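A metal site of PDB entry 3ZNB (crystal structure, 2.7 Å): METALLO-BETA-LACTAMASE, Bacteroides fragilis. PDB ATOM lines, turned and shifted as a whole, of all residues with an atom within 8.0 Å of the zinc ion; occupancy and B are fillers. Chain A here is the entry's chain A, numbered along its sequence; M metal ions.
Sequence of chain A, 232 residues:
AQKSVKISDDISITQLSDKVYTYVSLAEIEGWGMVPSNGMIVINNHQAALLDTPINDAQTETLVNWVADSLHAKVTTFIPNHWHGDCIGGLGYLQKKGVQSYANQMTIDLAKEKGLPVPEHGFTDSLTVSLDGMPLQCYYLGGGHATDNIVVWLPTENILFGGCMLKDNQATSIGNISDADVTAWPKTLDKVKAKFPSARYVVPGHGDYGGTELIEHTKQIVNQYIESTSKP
Residues that only touch the zinc ion: Asp 86 (3.9 Å).
Four residues have an atom within 4 Å of the zinc ion: His 82, His 84, Asp 86 and His 145.
The nearest printed residue that does not touch the zinc ion is Cys 164 (4.6 Å).
N of His 145 sits at hydrogen-bond distance from OD1 of Asn 149.
A ring nitrogen (NE2) of His 84 sits at hydrogen-bond distance from the side-chain carboxylate of Asp 179, 2.7 Å away.
The side-chain carboxylate of Asp 86 lies close to a ring nitrogen (NE2) of His 206 (3.1 Å).
The backbone carbonyl oxygen (O) of His 84 sits close to the side-chain sulfur (SG) of Cys 87, at 3.4 Å.
A ring nitrogen (ND1) of His 82 sits at hydrogen-bond distance from the side-chain amide oxygen of Asn 81, 2.6 Å away.
SG of Cys 87 sits close to O of His 82, at 3.3 Å.
SG of Cys 164 lies close to OD2 of Asp 86 (3.7 Å).
ND1 of His 84 binds the zinc ion.
NE2 of His 145 binds the zinc ion (2.3 Å).
NE2 of His 82 binds the zinc ion (2.4 Å).
The zinc ion has three donor atoms within binding distance.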
ATOM      1  N   ASP A  52      19.715  -9.452  14.775  1.00  0.00           N
ATOM      2  CA  ASP A  52      20.149 -10.317  13.646  1.00  0.00           C
ATOM      3  C   ASP A  52      19.920  -9.525  12.383  1.00  0.00           C
ATOM      4  O   ASP A  52      19.087  -8.642  12.348  1.00  0.00           O
ATOM      5  CB  ASP A  52      19.421 -11.703  13.586  1.00  0.00           C
ATOM      6  CG  ASP A  52      20.223 -12.847  14.258  1.00  0.00           C
ATOM      7  OD1 ASP A  52      20.945 -12.547  15.234  1.00  0.00           O
ATOM      8  OD2 ASP A  52      20.136 -14.042  13.819  1.00  0.00           O
ATOM      9  N   ASN A  81      22.981 -13.151  17.002  1.00  0.00           N
ATOM     10  CA  ASN A  81      22.772 -14.412  17.785  1.00  0.00           C
ATOM     11  C   ASN A  81      24.086 -15.191  17.920  1.00  0.00           C
ATOM     12  O   ASN A  81      24.420 -15.865  18.947  1.00  0.00           O
ATOM     13  CB  ASN A  81      21.704 -15.276  17.111  1.00  0.00           C
ATOM     14  CG  ASN A  81      21.388 -16.533  17.899  1.00  0.00           C
ATOM     15  OD1 ASN A  81      21.806 -17.650  17.548  1.00  0.00           O
ATOM     16  ND2 ASN A  81      20.577 -16.384  18.932  1.00  0.00           N
ATOM     17  N   HIS A  82      24.830 -15.140  16.828  1.00  0.00           N
ATOM     18  CA  HIS A  82      26.120 -15.782  16.752  1.00  0.00           C
ATOM     19  C   HIS A  82      26.707 -15.340  15.410  1.00  0.00           C
ATOM     20  O   HIS A  82      26.060 -14.560  14.653  1.00  0.00           O
ATOM     21  CB  HIS A  82      26.032 -17.279  16.949  1.00  0.00           C
ATOM     22  CG  HIS A  82      25.218 -17.991  15.915  1.00  0.00           C
ATOM     23  ND1 HIS A  82      23.846 -18.168  15.979  1.00  0.00           N
ATOM     24  CD2 HIS A  82      25.618 -18.584  14.761  1.00  0.00           C
ATOM     25  CE1 HIS A  82      23.453 -18.830  14.886  1.00  0.00           C
ATOM     26  NE2 HIS A  82      24.502 -19.105  14.118  1.00  0.00           N
ATOM     27  N   TRP A  83      27.946 -15.754  15.138  1.00  0.00           N
ATOM     28  CA  TRP A  83      28.666 -15.336  13.969  1.00  0.00           C
ATOM     29  C   TRP A  83      28.212 -15.754  12.560  1.00  0.00           C
ATOM     30  O   TRP A  83      28.736 -15.249  11.551  1.00  0.00           O
ATOM     31  CB  TRP A  83      30.118 -15.646  14.166  1.00  0.00           C
ATOM     32  CG  TRP A  83      30.399 -17.106  14.182  1.00  0.00           C
ATOM     33  CD1 TRP A  83      30.379 -17.927  15.274  1.00  0.00           C
ATOM     34  CD2 TRP A  83      30.736 -17.914  13.079  1.00  0.00           C
ATOM     35  NE1 TRP A  83      30.692 -19.205  14.908  1.00  0.00           N
ATOM     36  CE2 TRP A  83      30.916 -19.220  13.566  1.00  0.00           C
ATOM     37  CE3 TRP A  83      30.898 -17.667  11.712  1.00  0.00           C
ATOM     38  CZ2 TRP A  83      31.269 -20.289  12.703  1.00  0.00           C
ATOM     39  CZ3 TRP A  83      31.229 -18.720  10.884  1.00  0.00           C
ATOM     40  CH2 TRP A  83      31.423 -20.021  11.372  1.00  0.00           C
ATOM     41  N   HIS A  84      27.190 -16.601  12.448  1.00  0.00           N
ATOM     42  CA  HIS A  84      26.720 -17.023  11.138  1.00  0.00           C
ATOM     43  C   HIS A  84      26.094 -15.933  10.306  1.00  0.00           C
ATOM     44  O   HIS A  84      25.454 -15.043  10.834  1.00  0.00           O
ATOM     45  CB  HIS A  84      25.806 -18.229  11.220  1.00  0.00           C
ATOM     46  CG  HIS A  84      26.550 -19.492  11.504  1.00  0.00           C
ATOM     47  ND1 HIS A  84      25.953 -20.591  12.080  1.00  0.00           N
ATOM     48  CD2 HIS A  84      27.850 -19.814  11.336  1.00  0.00           C
ATOM     49  CE1 HIS A  84      26.860 -21.537  12.244  1.00  0.00           C
ATOM     50  NE2 HIS A  84      28.015 -21.081  11.814  1.00  0.00           N
ATOM     51  N   GLY A  85      26.290 -16.018   8.990  1.00  0.00           N
ATOM     52  CA  GLY A  85      25.768 -15.074   8.035  1.00  0.00           C
ATOM     53  C   GLY A  85      24.343 -14.660   8.202  1.00  0.00           C
ATOM     54  O   GLY A  85      24.043 -13.516   8.006  1.00  0.00           O
ATOM     55  N   ASP A  86      23.437 -15.566   8.538  1.00  0.00           N
ATOM     56  CA  ASP A  86      22.037 -15.178   8.710  1.00  0.00           C
ATOM     57  C   ASP A  86      21.854 -14.472  10.045  1.00  0.00           C
ATOM     58  O   ASP A  86      20.749 -14.386  10.524  1.00  0.00           O
ATOM     59  CB  ASP A  86      21.082 -16.379   8.578  1.00  0.00           C
ATOM     60  CG  ASP A  86      21.412 -17.557   9.530  1.00  0.00           C
ATOM     61  OD1 ASP A  86      22.601 -17.860   9.842  1.00  0.00           O
ATOM     62  OD2 ASP A  86      20.453 -18.231   9.978  1.00  0.00           O
ATOM     63  N   CYS A  87      22.969 -14.087  10.674  1.00  0.00           N
ATOM     64  CA  CYS A  87      22.963 -13.363  11.941  1.00  0.00           C
ATOM     65  C   CYS A  87      23.651 -12.071  11.753  1.00  0.00           C
ATOM     66  O   CYS A  87      23.219 -11.096  12.333  1.00  0.00           O
ATOM     67  CB  CYS A  87      23.773 -14.057  12.981  1.00  0.00           C
ATOM     68  SG  CYS A  87      23.221 -15.617  13.334  1.00  0.00           S
ATOM     69  N   HIS A 145      23.303 -24.425  18.977  1.00  0.00           N
ATOM     70  CA  HIS A 145      23.413 -24.531  17.543  1.00  0.00           C
ATOM     71  C   HIS A 145      24.771 -24.072  17.102  1.00  0.00           C
ATOM     72  O   HIS A 145      25.251 -24.426  16.055  1.00  0.00           O
ATOM     73  CB  HIS A 145      22.367 -23.666  16.922  1.00  0.00           C
ATOM     74  CG  HIS A 145      22.663 -23.309  15.515  1.00  0.00           C
ATOM     75  ND1 HIS A 145      22.464 -24.184  14.469  1.00  0.00           N
ATOM     76  CD2 HIS A 145      23.213 -22.190  14.975  1.00  0.00           C
ATOM     77  CE1 HIS A 145      22.880 -23.627  13.353  1.00  0.00           C
ATOM     78  NE2 HIS A 145      23.337 -22.419  13.633  1.00  0.00           N
ATOM     79  N   ALA A 146      25.349 -23.177  17.862  1.00  0.00           N
ATOM     80  CA  ALA A 146      26.688 -22.662  17.626  1.00  0.00           C
ATOM     81  C   ALA A 146      27.242 -22.469  19.057  1.00  0.00           C
ATOM     82  O   ALA A 146      26.487 -22.223  20.016  1.00  0.00           O
ATOM     83  CB  ALA A 146      26.653 -21.320  16.853  1.00  0.00           C
ATOM     84  N   ASP A 148      28.848 -20.053  20.309  1.00  0.00           N
ATOM     85  CA  ASP A 148      28.631 -18.724  20.870  1.00  0.00           C
ATOM     86  C   ASP A 148      27.200 -18.289  20.957  1.00  0.00           C
ATOM     87  O   ASP A 148      26.943 -17.208  21.451  1.00  0.00           O
ATOM     88  CB  ASP A 148      29.362 -17.684  20.077  1.00  0.00           C
ATOM     89  CG  ASP A 148      29.109 -17.807  18.588  1.00  0.00           C
ATOM     90  OD1 ASP A 148      28.912 -18.885  18.063  1.00  0.00           O
ATOM     91  OD2 ASP A 148      29.115 -16.777  17.890  1.00  0.00           O
ATOM     92  N   ASN A 149      26.268 -19.110  20.517  1.00  0.00           N
ATOM     93  CA  ASN A 149      24.884 -18.693  20.517  1.00  0.00           C
ATOM     94  C   ASN A 149      24.294 -18.128  21.824  1.00  0.00           C
ATOM     95  O   ASN A 149      24.456 -18.713  22.908  1.00  0.00           O
ATOM     96  CB  ASN A 149      23.984 -19.766  19.872  1.00  0.00           C
ATOM     97  CG  ASN A 149      23.911 -21.083  20.646  1.00  0.00           C
ATOM     98  OD1 ASN A 149      23.304 -22.039  20.149  1.00  0.00           O
ATOM     99  ND2 ASN A 149      24.475 -21.158  21.842  1.00  0.00           N
ATOM    100  N   CYS A 164      18.488 -19.097  16.505  1.00  0.00           N
ATOM    101  CA  CYS A 164      18.732 -20.305  15.737  1.00  0.00           C
ATOM    102  C   CYS A 164      18.996 -21.487  16.700  1.00  0.00           C
ATOM    103  O   CYS A 164      19.222 -22.591  16.302  1.00  0.00           O
ATOM    104  CB  CYS A 164      19.844 -20.051  14.710  1.00  0.00           C
ATOM    105  SG  CYS A 164      19.721 -18.451  13.564  1.00  0.00           S
ATOM    106  N   MET A 165      18.849 -21.250  17.973  1.00  0.00           N
ATOM    107  CA  MET A 165      19.023 -22.299  18.995  1.00  0.00           C
ATOM    108  C   MET A 165      17.701 -23.093  19.180  1.00  0.00           C
ATOM    109  O   MET A 165      17.667 -24.162  19.761  1.00  0.00           O
ATOM    110  CB  MET A 165      19.336 -21.621  20.285  1.00  0.00           C
ATOM    111  CG  MET A 165      19.618 -22.518  21.345  1.00  0.00           C
ATOM    112  SD  MET A 165      19.326 -21.594  22.802  1.00  0.00           S
ATOM    113  CE  MET A 165      20.913 -20.738  23.166  1.00  0.00           C
ATOM    114  N   ASN A 176      22.175 -27.662  10.423  1.00  0.00           N
ATOM    115  CA  ASN A 176      23.650 -27.515  10.335  1.00  0.00           C
ATOM    116  C   ASN A 176      24.322 -27.666  11.677  1.00  0.00           C
ATOM    117  O   ASN A 176      24.336 -26.725  12.489  1.00  0.00           O
ATOM    118  CB  ASN A 176      24.047 -26.166   9.732  1.00  0.00           C
ATOM    119  CG  ASN A 176      25.559 -25.945   9.752  1.00  0.00           C
ATOM    120  OD1 ASN A 176      26.302 -26.901   9.690  1.00  0.00           O
ATOM    121  ND2 ASN A 176      26.016 -24.683   9.850  1.00  0.00           N
ATOM    122  N   SER A 178      27.465 -28.062  12.110  1.00  0.00           N
ATOM    123  CA  SER A 178      28.903 -27.831  11.905  1.00  0.00           C
ATOM    124  C   SER A 178      29.511 -27.041  13.035  1.00  0.00           C
ATOM    125  O   SER A 178      30.632 -27.329  13.389  1.00  0.00           O
ATOM    126  CB  SER A 178      29.168 -27.080  10.596  1.00  0.00           C
ATOM    127  OG  SER A 178      28.423 -25.852  10.559  1.00  0.00           O
ATOM    128  N   ASP A 179      28.770 -26.086  13.601  1.00  0.00           N
ATOM    129  CA  ASP A 179      29.328 -25.240  14.653  1.00  0.00           C
ATOM    130  C   ASP A 179      28.539 -25.444  15.915  1.00  0.00           C
ATOM    131  O   ASP A 179      28.701 -24.701  16.878  1.00  0.00           O
ATOM    132  CB  ASP A 179      29.343 -23.754  14.235  1.00  0.00           C
ATOM    133  CG  ASP A 179      30.027 -23.527  12.858  1.00  0.00           C
ATOM    134  OD1 ASP A 179      31.270 -23.410  12.830  1.00  0.00           O
ATOM    135  OD2 ASP A 179      29.349 -23.477  11.799  1.00  0.00           O
ATOM    136  N   HIS A 206      14.413 -19.792  12.141  1.00  0.00           N
ATOM    137  CA  HIS A 206      13.771 -20.023  10.870  1.00  0.00           C
ATOM    138  C   HIS A 206      12.432 -20.587  11.218  1.00  0.00           C
ATOM    139  O   HIS A 206      12.327 -21.338  12.198  1.00  0.00           O
ATOM    140  CB  HIS A 206      14.577 -21.053  10.063  1.00  0.00           C
ATOM    141  CG  HIS A 206      16.009 -20.683   9.843  1.00  0.00           C
ATOM    142  ND1 HIS A 206      16.399 -19.604   9.068  1.00  0.00           N
ATOM    143  CD2 HIS A 206      17.132 -21.190  10.375  1.00  0.00           C
ATOM    144  CE1 HIS A 206      17.712 -19.462   9.153  1.00  0.00           C
ATOM    145  NE2 HIS A 206      18.179 -20.409   9.945  1.00  0.00           N
HETATM  146 ZN    ZN M   1      23.799 -20.596  12.352  1.00  0.00          ZN
HETATM  147 HG    HG M   2      21.195 -16.718  13.347  1.00  0.00          HG
